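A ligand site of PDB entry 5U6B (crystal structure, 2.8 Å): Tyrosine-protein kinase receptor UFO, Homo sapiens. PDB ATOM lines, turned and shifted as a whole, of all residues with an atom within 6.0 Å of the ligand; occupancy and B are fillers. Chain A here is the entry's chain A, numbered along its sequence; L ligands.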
ATOM      1  N   LEU A  31      -2.707  23.349 -28.219  1.00  0.00           N
ATOM      2  CA  LEU A  31      -3.922  22.757 -28.794  1.00  0.00           C
ATOM      3  C   LEU A  31      -5.097  22.739 -27.828  1.00  0.00           C
ATOM      4  O   LEU A  31      -6.245  22.683 -28.266  1.00  0.00           O
ATOM      5  CB  LEU A  31      -3.649  21.346 -29.357  1.00  0.00           C
ATOM      6  CG  LEU A  31      -2.521  21.188 -30.365  1.00  0.00           C
ATOM      7  CD1 LEU A  31      -2.228  19.738 -30.598  1.00  0.00           C
ATOM      8  CD2 LEU A  31      -2.843  21.847 -31.674  1.00  0.00           C
ATOM      9  N   GLY A  32      -4.815  22.816 -26.523  1.00  0.00           N
ATOM     10  CA  GLY A  32      -5.837  22.810 -25.492  1.00  0.00           C
ATOM     11  C   GLY A  32      -5.332  22.601 -24.084  1.00  0.00           C
ATOM     12  O   GLY A  32      -4.215  22.101 -23.883  1.00  0.00           O
ATOM     13  N   GLU A  33      -6.158  22.982 -23.100  1.00  0.00           N
ATOM     14  CA  GLU A  33      -5.875  22.874 -21.666  1.00  0.00           C
ATOM     15  C   GLU A  33      -6.821  21.915 -20.961  1.00  0.00           C
ATOM     16  O   GLU A  33      -7.987  21.781 -21.344  1.00  0.00           O
ATOM     17  CB  GLU A  33      -5.938  24.248 -20.983  1.00  0.00           C
ATOM     18  CG  GLU A  33      -4.938  24.426 -19.862  1.00  0.00           C
ATOM     19  CD  GLU A  33      -3.615  24.998 -20.334  1.00  0.00           C
ATOM     20  OE1 GLU A  33      -3.330  26.173 -20.005  1.00  0.00           O
ATOM     21  OE2 GLU A  33      -2.891  24.290 -21.072  1.00  0.00           O
ATOM     22  N   VAL A  39      -1.595  20.328 -23.757  1.00  0.00           N
ATOM     23  CA  VAL A  39      -1.256  19.678 -25.022  1.00  0.00           C
ATOM     24  C   VAL A  39      -0.806  20.737 -26.060  1.00  0.00           C
ATOM     25  O   VAL A  39      -1.515  21.735 -26.241  1.00  0.00           O
ATOM     26  CB  VAL A  39      -2.410  18.761 -25.550  1.00  0.00           C
ATOM     27  CG1 VAL A  39      -2.067  18.105 -26.885  1.00  0.00           C
ATOM     28  CG2 VAL A  39      -2.768  17.694 -24.526  1.00  0.00           C
ATOM     29  N   ALA A  54       1.836  15.570 -31.440  1.00  0.00           N
ATOM     30  CA  ALA A  54       1.023  16.098 -30.344  1.00  0.00           C
ATOM     31  C   ALA A  54       1.814  15.775 -29.085  1.00  0.00           C
ATOM     32  O   ALA A  54       2.326  14.659 -28.945  1.00  0.00           O
ATOM     33  CB  ALA A  54      -0.315  15.418 -30.315  1.00  0.00           C
ATOM     34  N   VAL A  55       2.003  16.762 -28.205  1.00  0.00           N
ATOM     35  CA  VAL A  55       2.824  16.623 -26.996  1.00  0.00           C
ATOM     36  C   VAL A  55       1.965  16.889 -25.771  1.00  0.00           C
ATOM     37  O   VAL A  55       1.612  18.036 -25.489  1.00  0.00           O
ATOM     38  CB  VAL A  55       4.082  17.566 -27.043  1.00  0.00           C
ATOM     39  CG1 VAL A  55       5.014  17.306 -25.869  1.00  0.00           C
ATOM     40  CG2 VAL A  55       4.837  17.465 -28.374  1.00  0.00           C
ATOM     41  N   LYS A  56       1.622  15.825 -25.028  1.00  0.00           N
ATOM     42  CA  LYS A  56       0.844  15.949 -23.797  1.00  0.00           C
ATOM     43  C   LYS A  56       1.783  15.823 -22.626  1.00  0.00           C
ATOM     44  O   LYS A  56       2.464  14.818 -22.487  1.00  0.00           O
ATOM     45  CB  LYS A  56      -0.284  14.898 -23.721  1.00  0.00           C
ATOM     46  CG  LYS A  56      -1.132  14.965 -22.442  1.00  0.00           C
ATOM     47  CD  LYS A  56      -2.562  14.508 -22.716  1.00  0.00           C
ATOM     48  CE  LYS A  56      -3.163  13.655 -21.646  1.00  0.00           C
ATOM     49  NZ  LYS A  56      -2.762  12.231 -21.800  1.00  0.00           N
ATOM     50  N   MET A  87      -4.774   4.523 -31.409  1.00  0.00           N
ATOM     51  CA  MET A  87      -3.719   5.538 -31.407  1.00  0.00           C
ATOM     52  C   MET A  87      -2.375   4.908 -31.142  1.00  0.00           C
ATOM     53  O   MET A  87      -2.217   4.183 -30.144  1.00  0.00           O
ATOM     54  CB  MET A  87      -4.020   6.621 -30.343  1.00  0.00           C
ATOM     55  CG  MET A  87      -2.940   7.670 -30.175  1.00  0.00           C
ATOM     56  SD  MET A  87      -3.087   8.899 -31.469  1.00  0.00           S
ATOM     57  CE  MET A  87      -3.956  10.116 -30.660  1.00  0.00           C
ATOM     58  N   LEU A 109       2.513  11.731 -29.176  1.00  0.00           N
ATOM     59  CA  LEU A 109       1.509  11.063 -30.035  1.00  0.00           C
ATOM     60  C   LEU A 109       1.555  11.584 -31.473  1.00  0.00           C
ATOM     61  O   LEU A 109       2.028  12.699 -31.688  1.00  0.00           O
ATOM     62  CB  LEU A 109       0.095  11.297 -29.454  1.00  0.00           C
ATOM     63  CG  LEU A 109      -0.126  10.925 -27.991  1.00  0.00           C
ATOM     64  CD1 LEU A 109      -1.354  11.562 -27.488  1.00  0.00           C
ATOM     65  CD2 LEU A 109      -0.181   9.425 -27.794  1.00  0.00           C
ATOM     66  N   PRO A 110       1.045  10.813 -32.479  1.00  0.00           N
ATOM     67  CA  PRO A 110       1.000  11.364 -33.849  1.00  0.00           C
ATOM     68  C   PRO A 110       0.051  12.540 -33.948  1.00  0.00           C
ATOM     69  O   PRO A 110      -0.946  12.600 -33.218  1.00  0.00           O
ATOM     70  CB  PRO A 110       0.488  10.195 -34.686  1.00  0.00           C
ATOM     71  CG  PRO A 110       0.634   8.984 -33.819  1.00  0.00           C
ATOM     72  CD  PRO A 110       0.440   9.475 -32.433  1.00  0.00           C
ATOM     73  N   PHE A 111       0.363  13.507 -34.811  1.00  0.00           N
ATOM     74  CA  PHE A 111      -0.497  14.670 -35.002  1.00  0.00           C
ATOM     75  C   PHE A 111      -1.708  14.335 -35.872  1.00  0.00           C
ATOM     76  O   PHE A 111      -1.561  14.034 -37.066  1.00  0.00           O
ATOM     77  CB  PHE A 111       0.288  15.869 -35.547  1.00  0.00           C
ATOM     78  CG  PHE A 111      -0.494  17.156 -35.524  1.00  0.00           C
ATOM     79  CD1 PHE A 111      -0.499  17.960 -34.394  1.00  0.00           C
ATOM     80  CD2 PHE A 111      -1.270  17.527 -36.608  1.00  0.00           C
ATOM     81  CE1 PHE A 111      -1.269  19.133 -34.356  1.00  0.00           C
ATOM     82  CE2 PHE A 111      -2.033  18.701 -36.563  1.00  0.00           C
ATOM     83  CZ  PHE A 111      -2.016  19.497 -35.439  1.00  0.00           C
ATOM     84  N   MET A 112      -2.905  14.370 -35.259  1.00  0.00           N
ATOM     85  CA  MET A 112      -4.208  14.119 -35.871  1.00  0.00           C
ATOM     86  C   MET A 112      -4.846  15.471 -36.163  1.00  0.00           C
ATOM     87  O   MET A 112      -5.429  16.084 -35.257  1.00  0.00           O
ATOM     88  CB  MET A 112      -5.099  13.334 -34.903  1.00  0.00           C
ATOM     89  CG  MET A 112      -5.432  11.955 -35.381  1.00  0.00           C
ATOM     90  SD  MET A 112      -4.116  10.794 -35.007  1.00  0.00           S
ATOM     91  CE  MET A 112      -4.718   9.378 -35.808  1.00  0.00           C
ATOM     92  N   LYS A 113      -4.704  15.955 -37.419  1.00  0.00           N
ATOM     93  CA  LYS A 113      -5.178  17.293 -37.804  1.00  0.00           C
ATOM     94  C   LYS A 113      -6.703  17.504 -37.687  1.00  0.00           C
ATOM     95  O   LYS A 113      -7.122  18.645 -37.468  1.00  0.00           O
ATOM     96  CB  LYS A 113      -4.677  17.704 -39.208  1.00  0.00           C
ATOM     97  CG  LYS A 113      -5.229  16.920 -40.391  1.00  0.00           C
ATOM     98  CD  LYS A 113      -5.110  17.737 -41.661  1.00  0.00           C
ATOM     99  CE  LYS A 113      -5.470  16.938 -42.882  1.00  0.00           C
ATOM    100  NZ  LYS A 113      -5.641  17.813 -44.053  1.00  0.00           N
ATOM    101  N   HIS A 114      -7.513  16.438 -37.787  1.00  0.00           N
ATOM    102  CA  HIS A 114      -8.961  16.571 -37.701  1.00  0.00           C
ATOM    103  C   HIS A 114      -9.512  16.620 -36.257  1.00  0.00           C
ATOM    104  O   HIS A 114     -10.733  16.736 -36.065  1.00  0.00           O
ATOM    105  CB  HIS A 114      -9.675  15.497 -38.543  1.00  0.00           C
ATOM    106  CG  HIS A 114      -9.286  15.513 -39.988  1.00  0.00           C
ATOM    107  ND1 HIS A 114      -9.716  16.515 -40.833  1.00  0.00           N
ATOM    108  CD2 HIS A 114      -8.476  14.677 -40.671  1.00  0.00           C
ATOM    109  CE1 HIS A 114      -9.166  16.244 -42.011  1.00  0.00           C
ATOM    110  NE2 HIS A 114      -8.415  15.141 -41.964  1.00  0.00           N
ATOM    111  N   GLY A 115      -8.604  16.574 -35.259  1.00  0.00           N
ATOM    112  CA  GLY A 115      -8.936  16.670 -33.836  1.00  0.00           C
ATOM    113  C   GLY A 115      -9.754  15.520 -33.275  1.00  0.00           C
ATOM    114  O   GLY A 115      -9.801  14.430 -33.868  1.00  0.00           O
ATOM    115  N   ASP A 116     -10.393  15.763 -32.111  1.00  0.00           N
ATOM    116  CA  ASP A 116     -11.198  14.747 -31.439  1.00  0.00           C
ATOM    117  C   ASP A 116     -12.598  14.603 -32.043  1.00  0.00           C
ATOM    118  O   ASP A 116     -13.136  15.568 -32.617  1.00  0.00           O
ATOM    119  CB  ASP A 116     -11.243  14.967 -29.908  1.00  0.00           C
ATOM    120  CG  ASP A 116     -12.160  16.082 -29.460  1.00  0.00           C
ATOM    121  OD1 ASP A 116     -13.355  15.801 -29.217  1.00  0.00           O
ATOM    122  OD2 ASP A 116     -11.666  17.221 -29.291  1.00  0.00           O
ATOM    123  N   LEU A 117     -13.181  13.398 -31.919  1.00  0.00           N
ATOM    124  CA  LEU A 117     -14.497  13.076 -32.440  1.00  0.00           C
ATOM    125  C   LEU A 117     -15.617  13.923 -31.816  1.00  0.00           C
ATOM    126  O   LEU A 117     -16.471  14.411 -32.573  1.00  0.00           O
ATOM    127  CB  LEU A 117     -14.763  11.564 -32.310  1.00  0.00           C
ATOM    128  CG  LEU A 117     -16.112  11.030 -32.845  1.00  0.00           C
ATOM    129  CD1 LEU A 117     -16.267  11.300 -34.337  1.00  0.00           C
ATOM    130  CD2 LEU A 117     -16.285   9.565 -32.516  1.00  0.00           C
ATOM    131  N   SER A 119     -15.624  17.050 -30.468  1.00  0.00           N
ATOM    132  CA  SER A 119     -15.540  18.412 -31.015  1.00  0.00           C
ATOM    133  C   SER A 119     -16.096  18.473 -32.447  1.00  0.00           C
ATOM    134  O   SER A 119     -16.879  19.374 -32.752  1.00  0.00           O
ATOM    135  CB  SER A 119     -14.097  18.914 -30.979  1.00  0.00           C
ATOM    136  OG  SER A 119     -13.637  19.046 -29.645  1.00  0.00           O
ATOM    137  N   ARG A 165     -14.892  12.045 -26.748  1.00  0.00           N
ATOM    138  CA  ARG A 165     -13.847  13.023 -26.470  1.00  0.00           C
ATOM    139  C   ARG A 165     -12.426  12.423 -26.501  1.00  0.00           C
ATOM    140  O   ARG A 165     -11.462  13.172 -26.664  1.00  0.00           O
ATOM    141  CB  ARG A 165     -14.119  13.728 -25.129  1.00  0.00           C
ATOM    142  CG  ARG A 165     -13.908  12.838 -23.913  1.00  0.00           C
ATOM    143  CD  ARG A 165     -14.048  13.548 -22.584  1.00  0.00           C
ATOM    144  NE  ARG A 165     -13.956  12.583 -21.490  1.00  0.00           N
ATOM    145  CZ  ARG A 165     -14.980  11.860 -21.033  1.00  0.00           C
ATOM    146  NH1 ARG A 165     -16.192  12.032 -21.544  1.00  0.00           N
ATOM    147  NH2 ARG A 165     -14.789  10.987 -20.053  1.00  0.00           N
ATOM    148  N   ASN A 166     -12.291  11.090 -26.283  1.00  0.00           N
ATOM    149  CA  ASN A 166     -11.014  10.377 -26.241  1.00  0.00           C
ATOM    150  C   ASN A 166     -10.808   9.538 -27.497  1.00  0.00           C
ATOM    151  O   ASN A 166     -10.039   8.569 -27.504  1.00  0.00           O
ATOM    152  CB  ASN A 166     -10.946   9.523 -24.963  1.00  0.00           C
ATOM    153  CG  ASN A 166     -10.808  10.310 -23.693  1.00  0.00           C
ATOM    154  OD1 ASN A 166     -10.180  11.371 -23.618  1.00  0.00           O
ATOM    155  ND2 ASN A 166     -11.366   9.775 -22.629  1.00  0.00           N
ATOM    156  N   CYS A 167     -11.523   9.908 -28.555  1.00  0.00           N
ATOM    157  CA  CYS A 167     -11.472   9.283 -29.857  1.00  0.00           C
ATOM    158  C   CYS A 167     -10.998  10.312 -30.825  1.00  0.00           C
ATOM    159  O   CYS A 167     -11.547  11.414 -30.838  1.00  0.00           O
ATOM    160  CB  CYS A 167     -12.844   8.755 -30.238  1.00  0.00           C
ATOM    161  SG  CYS A 167     -13.334   7.280 -29.318  1.00  0.00           S
ATOM    162  N   MET A 168      -9.936   9.970 -31.589  1.00  0.00           N
ATOM    163  CA  MET A 168      -9.303  10.850 -32.580  1.00  0.00           C
ATOM    164  C   MET A 168      -9.714  10.570 -34.040  1.00  0.00           C
ATOM    165  O   MET A 168     -10.064   9.438 -34.378  1.00  0.00           O
ATOM    166  CB  MET A 168      -7.776  10.834 -32.440  1.00  0.00           C
ATOM    167  CG  MET A 168      -7.283  11.475 -31.154  1.00  0.00           C
ATOM    168  SD  MET A 168      -7.921  13.140 -30.864  1.00  0.00           S
ATOM    169  CE  MET A 168      -6.904  14.038 -31.902  1.00  0.00           C
ATOM    170  N   ALA A 178      -8.188   6.494 -28.399  1.00  0.00           N
ATOM    171  CA  ALA A 178      -7.003   7.121 -27.783  1.00  0.00           C
ATOM    172  C   ALA A 178      -7.186   7.300 -26.277  1.00  0.00           C
ATOM    173  O   ALA A 178      -8.180   6.852 -25.734  1.00  0.00           O
ATOM    174  CB  ALA A 178      -6.729   8.461 -28.445  1.00  0.00           C
ATOM    175  N   ASP A 179      -6.198   7.928 -25.606  1.00  0.00           N
ATOM    176  CA  ASP A 179      -6.085   8.183 -24.162  1.00  0.00           C
ATOM    177  C   ASP A 179      -5.735   6.928 -23.384  1.00  0.00           C
ATOM    178  O   ASP A 179      -4.681   6.891 -22.743  1.00  0.00           O
ATOM    179  CB  ASP A 179      -7.313   8.896 -23.564  1.00  0.00           C
ATOM    180  CG  ASP A 179      -6.977   9.659 -22.296  1.00  0.00           C
ATOM    181  OD1 ASP A 179      -6.863   9.012 -21.230  1.00  0.00           O
ATOM    182  OD2 ASP A 179      -6.779  10.896 -22.383  1.00  0.00           O
HETATM  183  N1  LIG L   1      -3.493  15.035 -32.339  1.00  0.00           N
HETATM  184  C1  LIG L   1      -4.203  16.166 -32.383  1.00  0.00           C
HETATM  185  C2  LIG L   1      -4.803  16.714 -31.250  1.00  0.00           C
HETATM  186  C3  LIG L   1      -5.766  17.848 -31.323  1.00  0.00           C
HETATM  187  C4  LIG L   1      -5.872  18.841 -32.389  1.00  0.00           C
HETATM  188  C5  LIG L   1      -6.681  15.478 -27.106  1.00  0.00           C
HETATM  189  C6  LIG L   1      -4.230  14.893 -27.586  1.00  0.00           C
HETATM  190  C7  LIG L   1      -6.188  13.185 -27.505  1.00  0.00           C
HETATM  191  C8  LIG L   1      -7.506  12.857 -27.368  1.00  0.00           C
HETATM  192  C9  LIG L   1      -8.441  13.825 -27.080  1.00  0.00           C
HETATM  193  C10 LIG L   1      -8.497  20.050 -30.363  1.00  0.00           C
HETATM  194  C11 LIG L   1      -3.892  15.003 -30.002  1.00  0.00           C
HETATM  195  C12 LIG L   1      -3.326  14.386 -31.173  1.00  0.00           C
HETATM  196  N2  LIG L   1      -4.597  16.128 -30.050  1.00  0.00           N
HETATM  197  N3  LIG L   1      -6.826  19.711 -32.100  1.00  0.00           N
HETATM  198  N4  LIG L   1      -7.374  19.295 -30.909  1.00  0.00           N
HETATM  199  C13 LIG L   1      -6.769  18.189 -30.409  1.00  0.00           C
HETATM  200  C14 LIG L   1      -7.191  17.467 -29.148  1.00  0.00           C
HETATM  201  N5  LIG L   1      -6.524  17.796 -27.901  1.00  0.00           N
HETATM  202  C15 LIG L   1      -6.281  16.915 -26.915  1.00  0.00           C
HETATM  203  C16 LIG L   1      -5.718  14.495 -27.405  1.00  0.00           C
HETATM  204  O1  LIG L   1      -3.705  14.383 -28.813  1.00  0.00           O
HETATM  205  C17 LIG L   1      -3.334  14.414 -26.463  1.00  0.00           C
HETATM  206  C18 LIG L   1      -8.024  15.135 -26.933  1.00  0.00           C
HETATM  207  F1  LIG L   1      -7.909  11.583 -27.553  1.00  0.00           F
HETATM  208 CL1  LIG L   1      -5.101  11.877 -27.814  1.00  0.00          CL
HETATM  209  O2  LIG L   1      -5.781  17.233 -25.855  1.00  0.00           O
HETATM  210  C19 LIG L   1      -6.147  19.198 -27.704  1.00  0.00           C
HETATM  211  C20 LIG L   1      -9.793  19.801 -31.115  1.00  0.00           C
HETATM  212  O3  LIG L   1     -10.127  18.425 -31.137  1.00  0.00           O
HETATM  213  C21 LIG L   1      -5.102  18.980 -33.662  1.00  0.00           C
HETATM  214  N6  LIG L   1      -2.675  13.220 -31.184  1.00  0.00           N
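N of Asp 116 lies within hydrogen-bond range of O3 of the ligand. N1 of the ligand sits at hydrogen-bond distance from N of Met 112. OD2 of Asp 116 sits at hydrogen-bond distance from O3 of the ligand (2.7 Å). The backbone carbonyl oxygen (O) of Pro 110 is in hydrogen-bond range of a nitrogen (N6) of the ligand (2.7 Å).
The backbone NH (N) of Val 39 lies within hydrogen-bond range of the backbone carbonyl oxygen (O) of Gly 32. The backbone carbonyl oxygen of Asn 166 lies within hydrogen-bond range of the backbone NH of Ala 178. The backbone carbonyl oxygen (O) of Leu 109 sits at hydrogen-bond distance from the backbone NH (N) of Ala 54 (2.9 Å). The backbone carbonyl oxygen of Val 39 lies within hydrogen-bond range of the backbone NH of Leu 31 (2.8 Å). OD2 of Asp 116 sits at hydrogen-bond distance from OG of Ser 119, at 2.7 Å.
F1 of the ligand lies close to SD of Met 168 (3.7 Å). Merely in contact with the ligand: Arg 165 (3.1 Å), Ala 54 (3.3 Å), Val 39 (3.3 Å), Met 87 (3.4 Å), Gly 115 (3.4 Å), Ala 178 (3.5 Å), Leu 31 (3.5 Å), Asn 166 (3.5 Å), Phe 111 (3.6 Å), Leu 109 (3.6 Å), Lys 56 (3.8 Å) and Ser 119 (3.9 Å). Hydrophobic or aromatic side chains within 4 Å of the ligand: Leu 31, Val 39, Ala 54, Met 87, Leu 109, Phe 111, Met 112, Met 168 and Ala 178. Within 4 Å of the ligand: Leu 31, Val 39, Ala 54, Lys 56, Met 87, Leu 109, Pro 110, Phe 111, Met 112, Gly 115, Asp 116, Ser 119, Arg 165, Asn 166, Met 168 and Ala 178.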
